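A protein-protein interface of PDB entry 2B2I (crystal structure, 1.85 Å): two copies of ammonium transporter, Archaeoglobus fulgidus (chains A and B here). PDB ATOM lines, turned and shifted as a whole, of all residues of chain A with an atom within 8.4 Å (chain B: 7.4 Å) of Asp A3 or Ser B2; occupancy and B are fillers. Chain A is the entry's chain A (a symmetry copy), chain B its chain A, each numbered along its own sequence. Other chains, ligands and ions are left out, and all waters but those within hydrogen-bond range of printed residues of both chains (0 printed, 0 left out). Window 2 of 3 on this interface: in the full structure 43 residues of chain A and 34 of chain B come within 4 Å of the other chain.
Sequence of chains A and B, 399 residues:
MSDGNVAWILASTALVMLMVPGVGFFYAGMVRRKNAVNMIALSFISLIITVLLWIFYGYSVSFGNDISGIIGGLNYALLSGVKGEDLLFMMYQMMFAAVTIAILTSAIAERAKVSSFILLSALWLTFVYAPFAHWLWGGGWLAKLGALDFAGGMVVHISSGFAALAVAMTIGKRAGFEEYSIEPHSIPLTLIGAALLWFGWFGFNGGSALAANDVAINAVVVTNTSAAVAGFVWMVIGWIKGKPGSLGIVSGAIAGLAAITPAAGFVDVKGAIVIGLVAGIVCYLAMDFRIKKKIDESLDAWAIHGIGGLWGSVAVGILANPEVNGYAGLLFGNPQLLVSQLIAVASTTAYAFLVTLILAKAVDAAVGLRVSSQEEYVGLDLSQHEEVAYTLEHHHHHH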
ATOM      1  N   MET A   1      11.421   9.095   4.538  1.00  0.00           N
ATOM      2  CA  MET A   1      12.630   9.000   3.660  1.00  0.00           C
ATOM      3  C   MET A   1      13.213  10.373   3.398  1.00  0.00           C
ATOM      4  O   MET A   1      14.113  10.528   2.575  1.00  0.00           O
ATOM      5  CB  MET A   1      12.280   8.389   2.299  1.00  0.00           C
ATOM      6  CG  MET A   1      11.647   7.010   2.326  1.00  0.00           C
ATOM      7  SD  MET A   1      11.717   6.263   0.675  1.00  0.00           S
ATOM      8  CE  MET A   1      10.453   7.222  -0.217  1.00  0.00           C
ATOM      9  N   SER A   2      12.708  11.367   4.114  1.00  0.00           N
ATOM     10  CA  SER A   2      13.135  12.733   3.901  1.00  0.00           C
ATOM     11  C   SER A   2      12.496  13.045   2.566  1.00  0.00           C
ATOM     12  O   SER A   2      12.996  12.637   1.512  1.00  0.00           O
ATOM     13  CB  SER A   2      14.654  12.849   3.785  1.00  0.00           C
ATOM     14  OG  SER A   2      15.006  14.146   3.333  1.00  0.00           O
ATOM     15  N   ASP A   3      11.359  13.721   2.624  1.00  0.00           N
ATOM     16  CA  ASP A   3      10.661  14.101   1.421  1.00  0.00           C
ATOM     17  C   ASP A   3      11.572  15.041   0.655  1.00  0.00           C
ATOM     18  O   ASP A   3      11.563  15.070  -0.572  1.00  0.00           O
ATOM     19  CB  ASP A   3       9.353  14.797   1.779  1.00  0.00           C
ATOM     20  CG  ASP A   3       8.474  13.942   2.668  1.00  0.00           C
ATOM     21  OD1 ASP A   3       8.447  12.708   2.466  1.00  0.00           O
ATOM     22  OD2 ASP A   3       7.803  14.497   3.560  1.00  0.00           O
ATOM     23  N   GLY A   4      12.376  15.797   1.392  1.00  0.00           N
ATOM     24  CA  GLY A   4      13.277  16.730   0.755  1.00  0.00           C
ATOM     25  C   GLY A   4      14.219  16.008  -0.179  1.00  0.00           C
ATOM     26  O   GLY A   4      14.391  16.408  -1.336  1.00  0.00           O
ATOM     27  N   ASN A   5      14.822  14.932   0.319  1.00  0.00           N
ATOM     28  CA  ASN A   5      15.754  14.170  -0.491  1.00  0.00           C
ATOM     29  C   ASN A   5      15.068  13.538  -1.687  1.00  0.00           C
ATOM     30  O   ASN A   5      15.609  13.561  -2.793  1.00  0.00           O
ATOM     31  CB  ASN A   5      16.456  13.105   0.342  1.00  0.00           C
ATOM     32  CG  ASN A   5      17.458  13.701   1.307  1.00  0.00           C
ATOM     33  OD1 ASN A   5      17.782  14.893   1.232  1.00  0.00           O
ATOM     34  ND2 ASN A   5      17.962  12.880   2.215  1.00  0.00           N
ATOM     35  N   VAL A   6      13.880  12.974  -1.488  1.00  0.00           N
ATOM     36  CA  VAL A   6      13.169  12.388  -2.620  1.00  0.00           C
ATOM     37  C   VAL A   6      12.854  13.500  -3.620  1.00  0.00           C
ATOM     38  O   VAL A   6      13.043  13.332  -4.820  1.00  0.00           O
ATOM     39  CB  VAL A   6      11.842  11.700  -2.196  1.00  0.00           C
ATOM     40  CG1 VAL A   6      11.058  11.283  -3.430  1.00  0.00           C
ATOM     41  CG2 VAL A   6      12.142  10.475  -1.346  1.00  0.00           C
ATOM     42  N   ALA A   7      12.390  14.637  -3.108  1.00  0.00           N
ATOM     43  CA  ALA A   7      12.055  15.777  -3.945  1.00  0.00           C
ATOM     44  C   ALA A   7      13.217  16.104  -4.856  1.00  0.00           C
ATOM     45  O   ALA A   7      13.064  16.200  -6.074  1.00  0.00           O
ATOM     46  CB  ALA A   7      11.739  16.989  -3.085  1.00  0.00           C
ATOM     47  N   TRP A   8      14.385  16.268  -4.254  1.00  0.00           N
ATOM     48  CA  TRP A   8      15.557  16.628  -5.026  1.00  0.00           C
ATOM     49  C   TRP A   8      15.956  15.597  -6.065  1.00  0.00           C
ATOM     50  O   TRP A   8      16.354  15.959  -7.171  1.00  0.00           O
ATOM     51  CB  TRP A   8      16.733  16.923  -4.104  1.00  0.00           C
ATOM     52  CG  TRP A   8      17.944  17.313  -4.851  1.00  0.00           C
ATOM     53  CD1 TRP A   8      19.192  16.792  -4.706  1.00  0.00           C
ATOM     54  CD2 TRP A   8      18.028  18.274  -5.915  1.00  0.00           C
ATOM     55  NE1 TRP A   8      20.055  17.360  -5.613  1.00  0.00           N
ATOM     56  CE2 TRP A   8      19.367  18.275  -6.368  1.00  0.00           C
ATOM     57  CE3 TRP A   8      17.104  19.131  -6.530  1.00  0.00           C
ATOM     58  CZ2 TRP A   8      19.805  19.099  -7.412  1.00  0.00           C
ATOM     59  CZ3 TRP A   8      17.544  19.949  -7.567  1.00  0.00           C
ATOM     60  CH2 TRP A   8      18.884  19.923  -7.996  1.00  0.00           C
ATOM     61  N   ILE A   9      15.854  14.315  -5.741  1.00  0.00           N
ATOM     62  CA  ILE A   9      16.244  13.314  -6.730  1.00  0.00           C
ATOM     63  C   ILE A   9      15.199  13.134  -7.820  1.00  0.00           C
ATOM     64  O   ILE A   9      15.533  12.769  -8.953  1.00  0.00           O
ATOM     65  CB  ILE A   9      16.540  11.960  -6.092  1.00  0.00           C
ATOM     66  CG1 ILE A   9      17.619  12.124  -5.017  1.00  0.00           C
ATOM     67  CG2 ILE A   9      17.057  10.994  -7.145  1.00  0.00           C
ATOM     68  CD1 ILE A   9      18.912  12.758  -5.520  1.00  0.00           C
ATOM     69  N   LEU A  10      13.937  13.387  -7.488  1.00  0.00           N
ATOM     70  CA  LEU A  10      12.876  13.276  -8.481  1.00  0.00           C
ATOM     71  C   LEU A  10      13.164  14.366  -9.495  1.00  0.00           C
ATOM     72  O   LEU A  10      13.125  14.146 -10.705  1.00  0.00           O
ATOM     73  CB  LEU A  10      11.506  13.515  -7.843  1.00  0.00           C
ATOM     74  CG  LEU A  10      10.890  12.316  -7.103  1.00  0.00           C
ATOM     75  CD1 LEU A  10       9.653  12.733  -6.333  1.00  0.00           C
ATOM     76  CD2 LEU A  10      10.551  11.253  -8.123  1.00  0.00           C
ATOM     77  N   LEU A  88      13.865   4.701  -7.166  1.00  0.00           N
ATOM     78  CA  LEU A  88      14.240   6.055  -7.554  1.00  0.00           C
ATOM     79  C   LEU A  88      15.684   6.035  -8.052  1.00  0.00           C
ATOM     80  O   LEU A  88      16.028   6.717  -9.022  1.00  0.00           O
ATOM     81  CB  LEU A  88      14.084   7.032  -6.374  1.00  0.00           C
ATOM     82  CG  LEU A  88      14.397   8.522  -6.624  1.00  0.00           C
ATOM     83  CD1 LEU A  88      13.742   8.996  -7.902  1.00  0.00           C
ATOM     84  CD2 LEU A  88      13.923   9.353  -5.440  1.00  0.00           C
ATOM     85  N   ALA A 212      19.582  16.039  -0.702  1.00  0.00           N
ATOM     86  CA  ALA A 212      19.652  17.492  -0.746  1.00  0.00           C
ATOM     87  C   ALA A 212      20.457  17.891   0.482  1.00  0.00           C
ATOM     88  O   ALA A 212      19.888  18.293   1.488  1.00  0.00           O
ATOM     89  CB  ALA A 212      18.241  18.084  -0.688  1.00  0.00           C
ATOM     90  N   MET B   1       5.008  21.224   7.111  1.00  0.00           N
ATOM     91  CA  MET B   1       4.233  20.639   5.972  1.00  0.00           C
ATOM     92  C   MET B   1       5.102  19.704   5.155  1.00  0.00           C
ATOM     93  O   MET B   1       4.701  19.243   4.088  1.00  0.00           O
ATOM     94  CB  MET B   1       3.728  21.732   5.025  1.00  0.00           C
ATOM     95  CG  MET B   1       2.854  22.805   5.645  1.00  0.00           C
ATOM     96  SD  MET B   1       1.991  23.731   4.346  1.00  0.00           S
ATOM     97  CE  MET B   1       3.345  24.729   3.647  1.00  0.00           C
ATOM     98  N   SER B   2       6.287  19.411   5.669  1.00  0.00           N
ATOM     99  CA  SER B   2       7.232  18.588   4.946  1.00  0.00           C
ATOM    100  C   SER B   2       7.669  19.524   3.843  1.00  0.00           C
ATOM    101  O   SER B   2       6.954  19.717   2.853  1.00  0.00           O
ATOM    102  CB  SER B   2       6.570  17.351   4.341  1.00  0.00           C
ATOM    103  OG  SER B   2       7.466  16.714   3.446  1.00  0.00           O
ATOM    104  N   ASP B   3       8.819  20.148   4.047  1.00  0.00           N
ATOM    105  CA  ASP B   3       9.358  21.050   3.061  1.00  0.00           C
ATOM    106  C   ASP B   3       9.636  20.234   1.813  1.00  0.00           C
ATOM    107  O   ASP B   3       9.529  20.731   0.696  1.00  0.00           O
ATOM    108  CB  ASP B   3      10.643  21.681   3.584  1.00  0.00           C
ATOM    109  CG  ASP B   3      10.438  22.387   4.908  1.00  0.00           C
ATOM    110  OD1 ASP B   3       9.363  23.001   5.093  1.00  0.00           O
ATOM    111  OD2 ASP B   3      11.346  22.339   5.761  1.00  0.00           O
ATOM    112  N   GLY B   4       9.973  18.966   2.014  1.00  0.00           N
ATOM    113  CA  GLY B   4      10.264  18.108   0.888  1.00  0.00           C
ATOM    114  C   GLY B   4       9.073  18.022  -0.037  1.00  0.00           C
ATOM    115  O   GLY B   4       9.205  18.189  -1.255  1.00  0.00           O
ATOM    116  N   ASN B   5       7.902  17.771   0.542  1.00  0.00           N
ATOM    117  CA  ASN B   5       6.695  17.658  -0.256  1.00  0.00           C
ATOM    118  C   ASN B   5       6.356  18.966  -0.944  1.00  0.00           C
ATOM    119  O   ASN B   5       5.987  18.969  -2.119  1.00  0.00           O
ATOM    120  CB  ASN B   5       5.522  17.186   0.594  1.00  0.00           C
ATOM    121  CG  ASN B   5       5.649  15.730   0.987  1.00  0.00           C
ATOM    122  OD1 ASN B   5       6.509  15.005   0.472  1.00  0.00           O
ATOM    123  ND2 ASN B   5       4.792  15.287   1.894  1.00  0.00           N
ATOM    124  N   VAL B   6       6.477  20.085  -0.235  1.00  0.00           N
ATOM    125  CA  VAL B   6       6.197  21.368  -0.871  1.00  0.00           C
ATOM    126  C   VAL B   6       7.201  21.574  -2.004  1.00  0.00           C
ATOM    127  O   VAL B   6       6.831  21.981  -3.100  1.00  0.00           O
ATOM    128  CB  VAL B   6       6.305  22.559   0.121  1.00  0.00           C
ATOM    129  CG1 VAL B   6       6.195  23.873  -0.634  1.00  0.00           C
ATOM    130  CG2 VAL B   6       5.193  22.473   1.157  1.00  0.00           C
ATOM    131  N   ALA B   7       8.467  21.273  -1.729  1.00  0.00           N
ATOM    132  CA  ALA B   7       9.523  21.417  -2.717  1.00  0.00           C
ATOM    133  C   ALA B   7       9.133  20.710  -3.994  1.00  0.00           C
ATOM    134  O   ALA B   7       9.156  21.291  -5.079  1.00  0.00           O
ATOM    135  CB  ALA B   7      10.821  20.823  -2.194  1.00  0.00           C
ATOM    136  N   TRP B   8       8.765  19.444  -3.856  1.00  0.00           N
ATOM    137  CA  TRP B   8       8.412  18.657  -5.020  1.00  0.00           C
ATOM    138  C   TRP B   8       7.211  19.183  -5.784  1.00  0.00           C
ATOM    139  O   TRP B   8       7.205  19.162  -7.013  1.00  0.00           O
ATOM    140  CB  TRP B   8       8.188  17.201  -4.631  1.00  0.00           C
ATOM    141  CG  TRP B   8       7.845  16.361  -5.794  1.00  0.00           C
ATOM    142  CD1 TRP B   8       6.796  15.501  -5.894  1.00  0.00           C
ATOM    143  CD2 TRP B   8       8.516  16.330  -7.064  1.00  0.00           C
ATOM    144  NE1 TRP B   8       6.761  14.935  -7.147  1.00  0.00           N
ATOM    145  CE2 TRP B   8       7.806  15.426  -7.886  1.00  0.00           C
ATOM    146  CE3 TRP B   8       9.643  16.980  -7.588  1.00  0.00           C
ATOM    147  CZ2 TRP B   8       8.185  15.155  -9.207  1.00  0.00           C
ATOM    148  CZ3 TRP B   8      10.017  16.709  -8.900  1.00  0.00           C
ATOM    149  CH2 TRP B   8       9.287  15.804  -9.693  1.00  0.00           C
ATOM    150  N   GLU B  85      -1.416  25.125   1.909  1.00  0.00           N
ATOM    151  CA  GLU B  85      -1.225  24.200   0.809  1.00  0.00           C
ATOM    152  C   GLU B  85      -2.411  24.002  -0.112  1.00  0.00           C
ATOM    153  O   GLU B  85      -2.306  23.283  -1.106  1.00  0.00           O
ATOM    154  CB  GLU B  85      -0.699  22.843   1.288  1.00  0.00           C
ATOM    155  CG  GLU B  85      -1.239  22.305   2.579  1.00  0.00           C
ATOM    156  CD  GLU B  85      -0.563  20.981   2.939  1.00  0.00           C
ATOM    157  OE1 GLU B  85      -0.992  19.931   2.405  1.00  0.00           O
ATOM    158  OE2 GLU B  85       0.412  20.994   3.731  1.00  0.00           O
ATOM    159  N   ALA B 211       2.985  14.533  -3.131  1.00  0.00           N
ATOM    160  CA  ALA B 211       4.039  14.392  -2.134  1.00  0.00           C
ATOM    161  C   ALA B 211       5.221  13.674  -2.761  1.00  0.00           C
ATOM    162  O   ALA B 211       5.070  12.976  -3.767  1.00  0.00           O
ATOM    163  CB  ALA B 211       3.535  13.603  -0.927  1.00  0.00           C
ATOM    164  N   ALA B 212       6.396  13.857  -2.168  1.00  0.00           N
ATOM    165  CA  ALA B 212       7.612  13.218  -2.652  1.00  0.00           C
ATOM    166  C   ALA B 212       7.694  11.897  -1.903  1.00  0.00           C
ATOM    167  O   ALA B 212       8.433  11.783  -0.935  1.00  0.00           O
ATOM    168  CB  ALA B 212       8.825  14.099  -2.338  1.00  0.00           C
ATOM    169  N   ASN B 213       6.922  10.910  -2.360  1.00  0.00           N
ATOM    170  CA  ASN B 213       6.857   9.589  -1.727  1.00  0.00           C
ATOM    171  C   ASN B 213       6.991   8.413  -2.709  1.00  0.00           C
ATOM    172  O   ASN B 213       7.341   8.602  -3.881  1.00  0.00           O
ATOM    173  CB  ASN B 213       5.536   9.468  -0.965  1.00  0.00           C
ATOM    174  CG  ASN B 213       4.325   9.579  -1.875  1.00  0.00           C
ATOM    175  OD1 ASN B 213       3.189   9.651  -1.408  1.00  0.00           O
ATOM    176  ND2 ASN B 213       4.559   9.587  -3.180  1.00  0.00           N
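The side-chain amide oxygen (OD1) of Asn B5 sits close to the side-chain carboxylate (OD2) of Asp A3, 3.4 Å away.
OD2 of Asp A3 lies close to OG of Ser B2.
OG of Ser B2 sits at hydrogen-bond distance from N of Asn B5 (3.1 Å).
OD1 of Asn B5 sits at hydrogen-bond distance from N of Ala B212, at 2.9 Å.
Among the printed residues, merely in contact across the chains: Gly A4 with Gly B4, Asp A3 with Gly B4, Ala A7 with Gly B4, Asp A3 with Ala B212, Leu A10 with Trp B8, Val A6 with Ala B212, Ala A7 with Ala B212 and Ala A7 with Trp B8.
Of chain B, only Ser B2, Gly B4, Asn B5 and Ala B212 come within 4 Å of Asp A3.
Printed residues of chain B within 4 Å of Gly A4: Gly B4 (3.2 Å).
Gly B4 touches just these residues of chain A: Asp A3, Gly A4 and Ala A7.
Printed residues of chain B within 4 Å of Ala A7: Gly B4, Trp B8 and Ala B212.
Of the printed residues of chain A, Trp B8 touches Ala A7 (3.8 Å) and Leu A10 (3.6 Å).
Of the printed residues of chain A, Ala B212 touches Asp A3, Val A6 and Ala A7.
Printed residues of chain B within 4 Å of Val A6: Ala B212 (3.6 Å).
Printed residues of chain B within 4 Å of Leu A10: Trp B8 (3.6 Å).
The nearest residue of chain B that does not touch Asp A3 is Asn B213 (5.4 Å).
Hydrophobic or aromatic side chains of chain B that line the printed part of chain A: Trp B8 and Ala B212.
Printed residues of chain A that touch a printed residue of chain B: Asp A3, Gly A4, Val A6, Ala A7 and Leu A10.
Along chain A the printed residues that touch a printed residue of chain B span positions 3 to 10.
Among the printed residues, 10 pairs touch across the chains.
Among the printed residues, no Asp or Glu carboxylate lies within 4 Å of a Lys or Arg side-chain nitrogen of the other chain.
Asp A3 touches Ser B2, but with the chains exchanged Ser A2 does not touch Asp B3 (7.8 Å).
Asp A3 touches Gly B4, but with the chains exchanged Gly A4 does not touch Asp B3 (5.2 Å).
Asp A3 touches Asn B5, but with the chains exchanged Asn A5 does not touch Asp B3 (7.6 Å).
Gly A4 touches its own counterpart, Gly B4.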
